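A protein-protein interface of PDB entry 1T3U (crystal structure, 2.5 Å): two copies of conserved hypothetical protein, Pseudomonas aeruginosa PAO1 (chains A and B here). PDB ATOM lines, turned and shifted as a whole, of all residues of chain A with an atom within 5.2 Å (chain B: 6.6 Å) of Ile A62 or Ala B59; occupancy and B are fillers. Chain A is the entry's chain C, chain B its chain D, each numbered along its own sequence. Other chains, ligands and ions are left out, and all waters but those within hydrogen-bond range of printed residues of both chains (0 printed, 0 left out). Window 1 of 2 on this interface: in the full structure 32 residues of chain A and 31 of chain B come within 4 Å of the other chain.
O of Ala A59 lies within hydrogen-bond range of OG1 of Thr A63. O of Ala B59 sits at hydrogen-bond distance from OG1 of Thr B63 (2.8 Å).
Among the printed residues, pairs that only touch across the chains: Ala A31 with Thr B63, Leu A35 with Leu B60, Ala A59 with Leu B35, Ala A59 with Ala B55, Ala A59 with Ala B59, Leu A60 with Leu B35, Ile A62 with Ala B59, Thr A63 with Leu B35, Thr A63 with Ile B62, Leu A66 with Ile B62 and Leu A66 with Thr B63.
Printed residues of chain B within 4 Å of Ala A31: Thr B63 (3.8 Å). Printed residues of chain B within 4 Å of Leu A35: Leu B60. Ile A62 touches just one residue of chain B: Ala B59. His A64 touches none of the printed residues of chain B. Val B54 touches none of the printed residues of chain A. Of the printed residues of chain A, Ala B59 touches Ala A59 (3.8 Å) and Ile A62 (3.7 Å). Of the printed residues of chain A, Leu B60 touches Leu A35 (3.8 Å). The nearest residue of chain B that does not touch Ile A62 is Thr B63 (4.1 Å).
Of the 14 printed residues of chain A, 7 touch a printed residue of chain B. Printed residues of chain A that touch a printed residue of chain B: Ala A31, Leu A35, Ala A59, Leu A60, Ile A62, Thr A63 and Leu A66. Hydrophobic or aromatic side chains of chain A that line the printed part of chain B: Ala A31, Leu A35, Ala A59, Ile A62 and Leu A66. Of the 15 printed residues of chain B, 6 touch a printed residue of chain A. Among the printed residues, 11 pairs touch across the chains.
Leu A35 touches Leu B60, and with the chains exchanged Leu A60 touches Leu B35. Ile A62 touches Ala B59, but with the chains exchanged Ala A59 does not touch Ile B62 (5.8 Å). Thr A63 touches Leu B35, but with the chains exchanged Leu A35 does not touch Thr B63 (6.0 Å). Thr A63 touches Ile B62, but with the chains exchanged Ile A62 does not touch Thr B63 (4.1 Å).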
ATOM      1  N   ALA A  31     -26.133  28.235   8.891  1.00  0.00           N
ATOM      2  CA  ALA A  31     -26.055  27.094   9.777  1.00  0.00           C
ATOM      3  C   ALA A  31     -24.627  26.588   9.787  1.00  0.00           C
ATOM      4  O   ALA A  31     -24.071  26.273  10.842  1.00  0.00           O
ATOM      5  CB  ALA A  31     -27.005  26.002   9.306  1.00  0.00           C
ATOM      6  N   TYR A  34     -22.445  28.797  11.941  1.00  0.00           N
ATOM      7  CA  TYR A  34     -22.711  28.590  13.362  1.00  0.00           C
ATOM      8  C   TYR A  34     -21.972  27.340  13.814  1.00  0.00           C
ATOM      9  O   TYR A  34     -21.322  27.343  14.854  1.00  0.00           O
ATOM     10  CB  TYR A  34     -24.211  28.403  13.606  1.00  0.00           C
ATOM     11  CG  TYR A  34     -24.569  27.898  14.985  1.00  0.00           C
ATOM     12  CD1 TYR A  34     -25.101  28.748  15.944  1.00  0.00           C
ATOM     13  CD2 TYR A  34     -24.383  26.558  15.325  1.00  0.00           C
ATOM     14  CE1 TYR A  34     -25.445  28.274  17.206  1.00  0.00           C
ATOM     15  CE2 TYR A  34     -24.720  26.077  16.577  1.00  0.00           C
ATOM     16  CZ  TYR A  34     -25.254  26.933  17.514  1.00  0.00           C
ATOM     17  OH  TYR A  34     -25.618  26.436  18.749  1.00  0.00           O
ATOM     18  N   LEU A  35     -22.080  26.270  13.036  1.00  0.00           N
ATOM     19  CA  LEU A  35     -21.408  25.027  13.388  1.00  0.00           C
ATOM     20  C   LEU A  35     -19.904  25.216  13.383  1.00  0.00           C
ATOM     21  O   LEU A  35     -19.201  24.816  14.319  1.00  0.00           O
ATOM     22  CB  LEU A  35     -21.776  23.915  12.406  1.00  0.00           C
ATOM     23  CG  LEU A  35     -23.182  23.358  12.542  1.00  0.00           C
ATOM     24  CD1 LEU A  35     -23.538  22.597  11.282  1.00  0.00           C
ATOM     25  CD2 LEU A  35     -23.270  22.470  13.779  1.00  0.00           C
ATOM     26  N   ALA A  58     -21.285  20.076  18.739  1.00  0.00           N
ATOM     27  CA  ALA A  58     -21.695  21.225  17.950  1.00  0.00           C
ATOM     28  C   ALA A  58     -23.117  20.969  17.464  1.00  0.00           C
ATOM     29  O   ALA A  58     -24.002  21.797  17.625  1.00  0.00           O
ATOM     30  CB  ALA A  58     -20.764  21.407  16.760  1.00  0.00           C
ATOM     31  N   ALA A  59     -23.322  19.802  16.869  1.00  0.00           N
ATOM     32  CA  ALA A  59     -24.624  19.419  16.354  1.00  0.00           C
ATOM     33  C   ALA A  59     -25.699  19.435  17.432  1.00  0.00           C
ATOM     34  O   ALA A  59     -26.836  19.800  17.170  1.00  0.00           O
ATOM     35  CB  ALA A  59     -24.544  18.043  15.731  1.00  0.00           C
ATOM     36  N   LEU A  60     -25.350  19.032  18.645  1.00  0.00           N
ATOM     37  CA  LEU A  60     -26.339  19.015  19.703  1.00  0.00           C
ATOM     38  C   LEU A  60     -26.667  20.446  20.089  1.00  0.00           C
ATOM     39  O   LEU A  60     -27.799  20.766  20.445  1.00  0.00           O
ATOM     40  CB  LEU A  60     -25.821  18.227  20.918  1.00  0.00           C
ATOM     41  CG  LEU A  60     -26.712  18.252  22.168  1.00  0.00           C
ATOM     42  CD1 LEU A  60     -28.036  17.593  21.860  1.00  0.00           C
ATOM     43  CD2 LEU A  60     -26.017  17.553  23.335  1.00  0.00           C
ATOM     44  N   ASN A  61     -25.683  21.324  19.995  1.00  0.00           N
ATOM     45  CA  ASN A  61     -25.919  22.708  20.356  1.00  0.00           C
ATOM     46  C   ASN A  61     -26.850  23.413  19.365  1.00  0.00           C
ATOM     47  O   ASN A  61     -27.671  24.247  19.755  1.00  0.00           O
ATOM     48  CB  ASN A  61     -24.604  23.457  20.434  1.00  0.00           C
ATOM     49  CG  ASN A  61     -24.623  24.522  21.490  1.00  0.00           C
ATOM     50  OD1 ASN A  61     -25.482  25.404  21.481  1.00  0.00           O
ATOM     51  ND2 ASN A  61     -23.684  24.442  22.423  1.00  0.00           N
ATOM     52  N   ILE A  62     -26.710  23.066  18.088  1.00  0.00           N
ATOM     53  CA  ILE A  62     -27.519  23.635  17.019  1.00  0.00           C
ATOM     54  C   ILE A  62     -28.917  22.994  17.004  1.00  0.00           C
ATOM     55  O   ILE A  62     -29.906  23.653  16.701  1.00  0.00           O
ATOM     56  CB  ILE A  62     -26.811  23.437  15.647  1.00  0.00           C
ATOM     57  CG1 ILE A  62     -26.944  24.704  14.786  1.00  0.00           C
ATOM     58  CG2 ILE A  62     -27.381  22.236  14.914  1.00  0.00           C
ATOM     59  CD1 ILE A  62     -28.284  24.940  14.202  1.00  0.00           C
ATOM     60  N   THR A  63     -29.006  21.714  17.332  1.00  0.00           N
ATOM     61  CA  THR A  63     -30.301  21.065  17.342  1.00  0.00           C
ATOM     62  C   THR A  63     -31.093  21.648  18.492  1.00  0.00           C
ATOM     63  O   THR A  63     -32.309  21.765  18.429  1.00  0.00           O
ATOM     64  CB  THR A  63     -30.172  19.555  17.548  1.00  0.00           C
ATOM     65  OG1 THR A  63     -29.481  18.984  16.436  1.00  0.00           O
ATOM     66  CG2 THR A  63     -31.540  18.907  17.671  1.00  0.00           C
ATOM     67  N   HIS A  64     -30.381  22.015  19.549  1.00  0.00           N
ATOM     68  CA  HIS A  64     -31.000  22.589  20.730  1.00  0.00           C
ATOM     69  C   HIS A  64     -31.626  23.960  20.443  1.00  0.00           C
ATOM     70  O   HIS A  64     -32.719  24.241  20.917  1.00  0.00           O
ATOM     71  CB  HIS A  64     -29.961  22.710  21.847  1.00  0.00           C
ATOM     72  CG  HIS A  64     -30.522  23.207  23.140  1.00  0.00           C
ATOM     73  ND1 HIS A  64     -31.431  22.487  23.882  1.00  0.00           N
ATOM     74  CD2 HIS A  64     -30.326  24.368  23.810  1.00  0.00           C
ATOM     75  CE1 HIS A  64     -31.773  23.181  24.953  1.00  0.00           C
ATOM     76  NE2 HIS A  64     -31.116  24.328  24.931  1.00  0.00           N
ATOM     77  N   ASP A  65     -30.945  24.814  19.682  1.00  0.00           N
ATOM     78  CA  ASP A  65     -31.506  26.118  19.381  1.00  0.00           C
ATOM     79  C   ASP A  65     -32.644  25.960  18.392  1.00  0.00           C
ATOM     80  O   ASP A  65     -33.657  26.636  18.511  1.00  0.00           O
ATOM     81  CB  ASP A  65     -30.456  27.069  18.805  1.00  0.00           C
ATOM     82  CG  ASP A  65     -29.308  27.323  19.756  1.00  0.00           C
ATOM     83  OD1 ASP A  65     -29.521  27.221  20.990  1.00  0.00           O
ATOM     84  OD2 ASP A  65     -28.185  27.637  19.276  1.00  0.00           O
ATOM     85  N   LEU A  66     -32.477  25.060  17.426  1.00  0.00           N
ATOM     86  CA  LEU A  66     -33.496  24.810  16.405  1.00  0.00           C
ATOM     87  C   LEU A  66     -34.815  24.302  16.968  1.00  0.00           C
ATOM     88  O   LEU A  66     -35.878  24.644  16.456  1.00  0.00           O
ATOM     89  CB  LEU A  66     -32.986  23.822  15.357  1.00  0.00           C
ATOM     90  CG  LEU A  66     -31.895  24.366  14.445  1.00  0.00           C
ATOM     91  CD1 LEU A  66     -31.507  23.303  13.441  1.00  0.00           C
ATOM     92  CD2 LEU A  66     -32.398  25.613  13.732  1.00  0.00           C
ATOM     93  N   LEU A  67     -34.761  23.477  18.007  1.00  0.00           N
ATOM     94  CA  LEU A  67     -36.000  22.992  18.590  1.00  0.00           C
ATOM     95  C   LEU A  67     -36.703  24.134  19.318  1.00  0.00           C
ATOM     96  O   LEU A  67     -37.930  24.161  19.388  1.00  0.00           O
ATOM     97  CB  LEU A  67     -35.747  21.844  19.562  1.00  0.00           C
ATOM     98  CG  LEU A  67     -35.357  20.494  18.967  1.00  0.00           C
ATOM     99  CD1 LEU A  67     -35.295  19.473  20.109  1.00  0.00           C
ATOM    100  CD2 LEU A  67     -36.359  20.055  17.900  1.00  0.00           C
ATOM    101  N   ARG A  69     -36.537  27.256  18.370  1.00  0.00           N
ATOM    102  CA  ARG A  69     -37.094  28.080  17.316  1.00  0.00           C
ATOM    103  C   ARG A  69     -38.339  27.378  16.790  1.00  0.00           C
ATOM    104  O   ARG A  69     -39.305  28.022  16.388  1.00  0.00           O
ATOM    105  CB  ARG A  69     -36.071  28.298  16.194  1.00  0.00           C
ATOM    106  CG  ARG A  69     -35.053  29.399  16.500  1.00  0.00           C
ATOM    107  CD  ARG A  69     -33.744  29.220  15.716  1.00  0.00           C
ATOM    108  NE  ARG A  69     -32.683  30.101  16.208  1.00  0.00           N
ATOM    109  CZ  ARG A  69     -31.381  29.832  16.131  1.00  0.00           C
ATOM    110  NH1 ARG A  69     -30.955  28.701  15.579  1.00  0.00           N
ATOM    111  NH2 ARG A  69     -30.493  30.699  16.610  1.00  0.00           N
ATOM    112  N   LEU B  35     -31.196  14.274  17.535  1.00  0.00           N
ATOM    113  CA  LEU B  35     -29.903  14.204  16.843  1.00  0.00           C
ATOM    114  C   LEU B  35     -29.547  12.746  16.572  1.00  0.00           C
ATOM    115  O   LEU B  35     -29.264  12.367  15.433  1.00  0.00           O
ATOM    116  CB  LEU B  35     -28.800  14.844  17.700  1.00  0.00           C
ATOM    117  CG  LEU B  35     -27.656  15.622  17.030  1.00  0.00           C
ATOM    118  CD1 LEU B  35     -26.397  15.471  17.852  1.00  0.00           C
ATOM    119  CD2 LEU B  35     -27.409  15.159  15.626  1.00  0.00           C
ATOM    120  N   LYS B  38     -31.305  11.214  13.578  1.00  0.00           N
ATOM    121  CA  LYS B  38     -30.861  11.562  12.237  1.00  0.00           C
ATOM    122  C   LYS B  38     -29.505  10.986  11.886  1.00  0.00           C
ATOM    123  O   LYS B  38     -29.287  10.569  10.754  1.00  0.00           O
ATOM    124  CB  LYS B  38     -30.856  13.078  12.047  1.00  0.00           C
ATOM    125  CG  LYS B  38     -32.251  13.674  11.926  1.00  0.00           C
ATOM    126  CD  LYS B  38     -33.092  12.923  10.893  1.00  0.00           C
ATOM    127  CE  LYS B  38     -34.361  13.682  10.536  1.00  0.00           C
ATOM    128  NZ  LYS B  38     -34.075  14.820   9.616  1.00  0.00           N
ATOM    129  N   MET B  39     -28.589  10.965  12.847  1.00  0.00           N
ATOM    130  CA  MET B  39     -27.266  10.408  12.593  1.00  0.00           C
ATOM    131  C   MET B  39     -27.376   8.933  12.233  1.00  0.00           C
ATOM    132  O   MET B  39     -26.640   8.443  11.378  1.00  0.00           O
ATOM    133  CB  MET B  39     -26.362  10.580  13.812  1.00  0.00           C
ATOM    134  CG  MET B  39     -25.632  11.897  13.827  1.00  0.00           C
ATOM    135  SD  MET B  39     -24.627  12.174  15.432  1.00  0.00           S
ATOM    136  CE  MET B  39     -26.105  12.466  16.595  1.00  0.00           C
ATOM    137  N   ILE B  42     -28.557   8.642   8.639  1.00  0.00           N
ATOM    138  CA  ILE B  42     -27.463   9.007   7.750  1.00  0.00           C
ATOM    139  C   ILE B  42     -26.402   7.924   7.680  1.00  0.00           C
ATOM    140  O   ILE B  42     -25.732   7.771   6.657  1.00  0.00           O
ATOM    141  CB  ILE B  42     -26.778  10.305   8.180  1.00  0.00           C
ATOM    142  CG1 ILE B  42     -27.777  11.459   8.141  1.00  0.00           C
ATOM    143  CG2 ILE B  42     -25.592  10.577   7.268  1.00  0.00           C
ATOM    144  CD1 ILE B  42     -27.228  12.763   8.694  1.00  0.00           C
ATOM    145  N   VAL B  54     -20.895  12.613   9.873  1.00  0.00           N
ATOM    146  CA  VAL B  54     -22.266  12.200  10.096  1.00  0.00           C
ATOM    147  C   VAL B  54     -22.969  13.163  11.036  1.00  0.00           C
ATOM    148  O   VAL B  54     -24.163  13.410  10.907  1.00  0.00           O
ATOM    149  CB  VAL B  54     -22.321  10.773  10.664  1.00  0.00           C
ATOM    150  CG1 VAL B  54     -23.747  10.421  11.075  1.00  0.00           C
ATOM    151  CG2 VAL B  54     -21.822   9.794   9.613  1.00  0.00           C
ATOM    152  N   ALA B  55     -22.229  13.716  11.987  1.00  0.00           N
ATOM    153  CA  ALA B  55     -22.816  14.668  12.923  1.00  0.00           C
ATOM    154  C   ALA B  55     -23.071  16.002  12.202  1.00  0.00           C
ATOM    155  O   ALA B  55     -24.113  16.622  12.400  1.00  0.00           O
ATOM    156  CB  ALA B  55     -21.898  14.876  14.126  1.00  0.00           C
ATOM    157  N   VAL B  56     -22.125  16.434  11.364  1.00  0.00           N
ATOM    158  CA  VAL B  56     -22.284  17.683  10.636  1.00  0.00           C
ATOM    159  C   VAL B  56     -23.444  17.634   9.643  1.00  0.00           C
ATOM    160  O   VAL B  56     -24.180  18.610   9.496  1.00  0.00           O
ATOM    161  CB  VAL B  56     -20.996  18.070   9.891  1.00  0.00           C
ATOM    162  CG1 VAL B  56     -21.249  19.294   9.018  1.00  0.00           C
ATOM    163  CG2 VAL B  56     -19.898  18.362  10.895  1.00  0.00           C
ATOM    164  N   MET B  57     -23.614  16.501   8.971  1.00  0.00           N
ATOM    165  CA  MET B  57     -24.702  16.344   8.017  1.00  0.00           C
ATOM    166  C   MET B  57     -26.033  16.262   8.753  1.00  0.00           C
ATOM    167  O   MET B  57     -27.043  16.785   8.284  1.00  0.00           O
ATOM    168  CB  MET B  57     -24.505  15.084   7.176  1.00  0.00           C
ATOM    169  CG  MET B  57     -23.407  15.199   6.141  1.00  0.00           C
ATOM    170  SD  MET B  57     -23.815  16.565   4.832  1.00  0.00           S
ATOM    171  CE  MET B  57     -24.791  15.487   3.567  1.00  0.00           C
ATOM    172  N   ALA B  58     -26.027  15.609   9.911  1.00  0.00           N
ATOM    173  CA  ALA B  58     -27.234  15.461  10.717  1.00  0.00           C
ATOM    174  C   ALA B  58     -27.744  16.811  11.191  1.00  0.00           C
ATOM    175  O   ALA B  58     -28.948  17.037  11.235  1.00  0.00           O
ATOM    176  CB  ALA B  58     -26.953  14.564  11.918  1.00  0.00           C
ATOM    177  N   ALA B  59     -26.823  17.689  11.570  1.00  0.00           N
ATOM    178  CA  ALA B  59     -27.167  19.026  12.030  1.00  0.00           C
ATOM    179  C   ALA B  59     -27.689  19.865  10.853  1.00  0.00           C
ATOM    180  O   ALA B  59     -28.523  20.737  11.024  1.00  0.00           O
ATOM    181  CB  ALA B  59     -25.945  19.695  12.646  1.00  0.00           C
ATOM    182  N   LEU B  60     -27.185  19.582   9.660  1.00  0.00           N
ATOM    183  CA  LEU B  60     -27.591  20.295   8.464  1.00  0.00           C
ATOM    184  C   LEU B  60     -28.989  19.859   8.021  1.00  0.00           C
ATOM    185  O   LEU B  60     -29.796  20.693   7.608  1.00  0.00           O
ATOM    186  CB  LEU B  60     -26.583  20.037   7.351  1.00  0.00           C
ATOM    187  CG  LEU B  60     -25.552  21.100   6.968  1.00  0.00           C
ATOM    188  CD1 LEU B  60     -25.375  22.159   8.035  1.00  0.00           C
ATOM    189  CD2 LEU B  60     -24.263  20.394   6.660  1.00  0.00           C
ATOM    190  N   ASN B  61     -29.278  18.560   8.117  1.00  0.00           N
ATOM    191  CA  ASN B  61     -30.579  18.033   7.741  1.00  0.00           C
ATOM    192  C   ASN B  61     -31.617  18.581   8.697  1.00  0.00           C
ATOM    193  O   ASN B  61     -32.671  19.056   8.284  1.00  0.00           O
ATOM    194  CB  ASN B  61     -30.589  16.506   7.812  1.00  0.00           C
ATOM    195  CG  ASN B  61     -29.899  15.861   6.636  1.00  0.00           C
ATOM    196  OD1 ASN B  61     -28.712  16.061   6.402  1.00  0.00           O
ATOM    197  ND2 ASN B  61     -30.647  15.079   5.884  1.00  0.00           N
ATOM    198  N   ILE B  62     -31.313  18.520   9.983  1.00  0.00           N
ATOM    199  CA  ILE B  62     -32.243  19.028  10.973  1.00  0.00           C
ATOM    200  C   ILE B  62     -32.501  20.511  10.688  1.00  0.00           C
ATOM    201  O   ILE B  62     -33.614  21.008  10.887  1.00  0.00           O
ATOM    202  CB  ILE B  62     -31.690  18.835  12.384  1.00  0.00           C
ATOM    203  CG1 ILE B  62     -31.567  17.324  12.672  1.00  0.00           C
ATOM    204  CG2 ILE B  62     -32.586  19.521  13.392  1.00  0.00           C
ATOM    205  CD1 ILE B  62     -30.852  16.987  13.985  1.00  0.00           C
ATOM    206  N   THR B  63     -31.482  21.215  10.199  1.00  0.00           N
ATOM    207  CA  THR B  63     -31.654  22.622   9.873  1.00  0.00           C
ATOM    208  C   THR B  63     -32.613  22.729   8.688  1.00  0.00           C
ATOM    209  O   THR B  63     -33.622  23.443   8.739  1.00  0.00           O
ATOM    210  CB  THR B  63     -30.322  23.281   9.507  1.00  0.00           C
ATOM    211  OG1 THR B  63     -29.489  23.334  10.668  1.00  0.00           O
ATOM    212  CG2 THR B  63     -30.548  24.705   9.006  1.00  0.00           C
ATOM    213  N   HIS B  64     -32.288  22.014   7.624  1.00  0.00           N
ATOM    214  CA  HIS B  64     -33.120  22.003   6.442  1.00  0.00           C
ATOM    215  C   HIS B  64     -34.565  21.635   6.800  1.00  0.00           C
ATOM    216  O   HIS B  64     -35.507  22.193   6.241  1.00  0.00           O
ATOM    217  CB  HIS B  64     -32.569  20.989   5.451  1.00  0.00           C
ATOM    218  CG  HIS B  64     -33.528  20.631   4.358  1.00  0.00           C
ATOM    219  ND1 HIS B  64     -33.663  21.377   3.210  1.00  0.00           N
ATOM    220  CD2 HIS B  64     -34.389  19.589   4.235  1.00  0.00           C
ATOM    221  CE1 HIS B  64     -34.563  20.810   2.422  1.00  0.00           C
ATOM    222  NE2 HIS B  64     -35.017  19.723   3.023  1.00  0.00           N
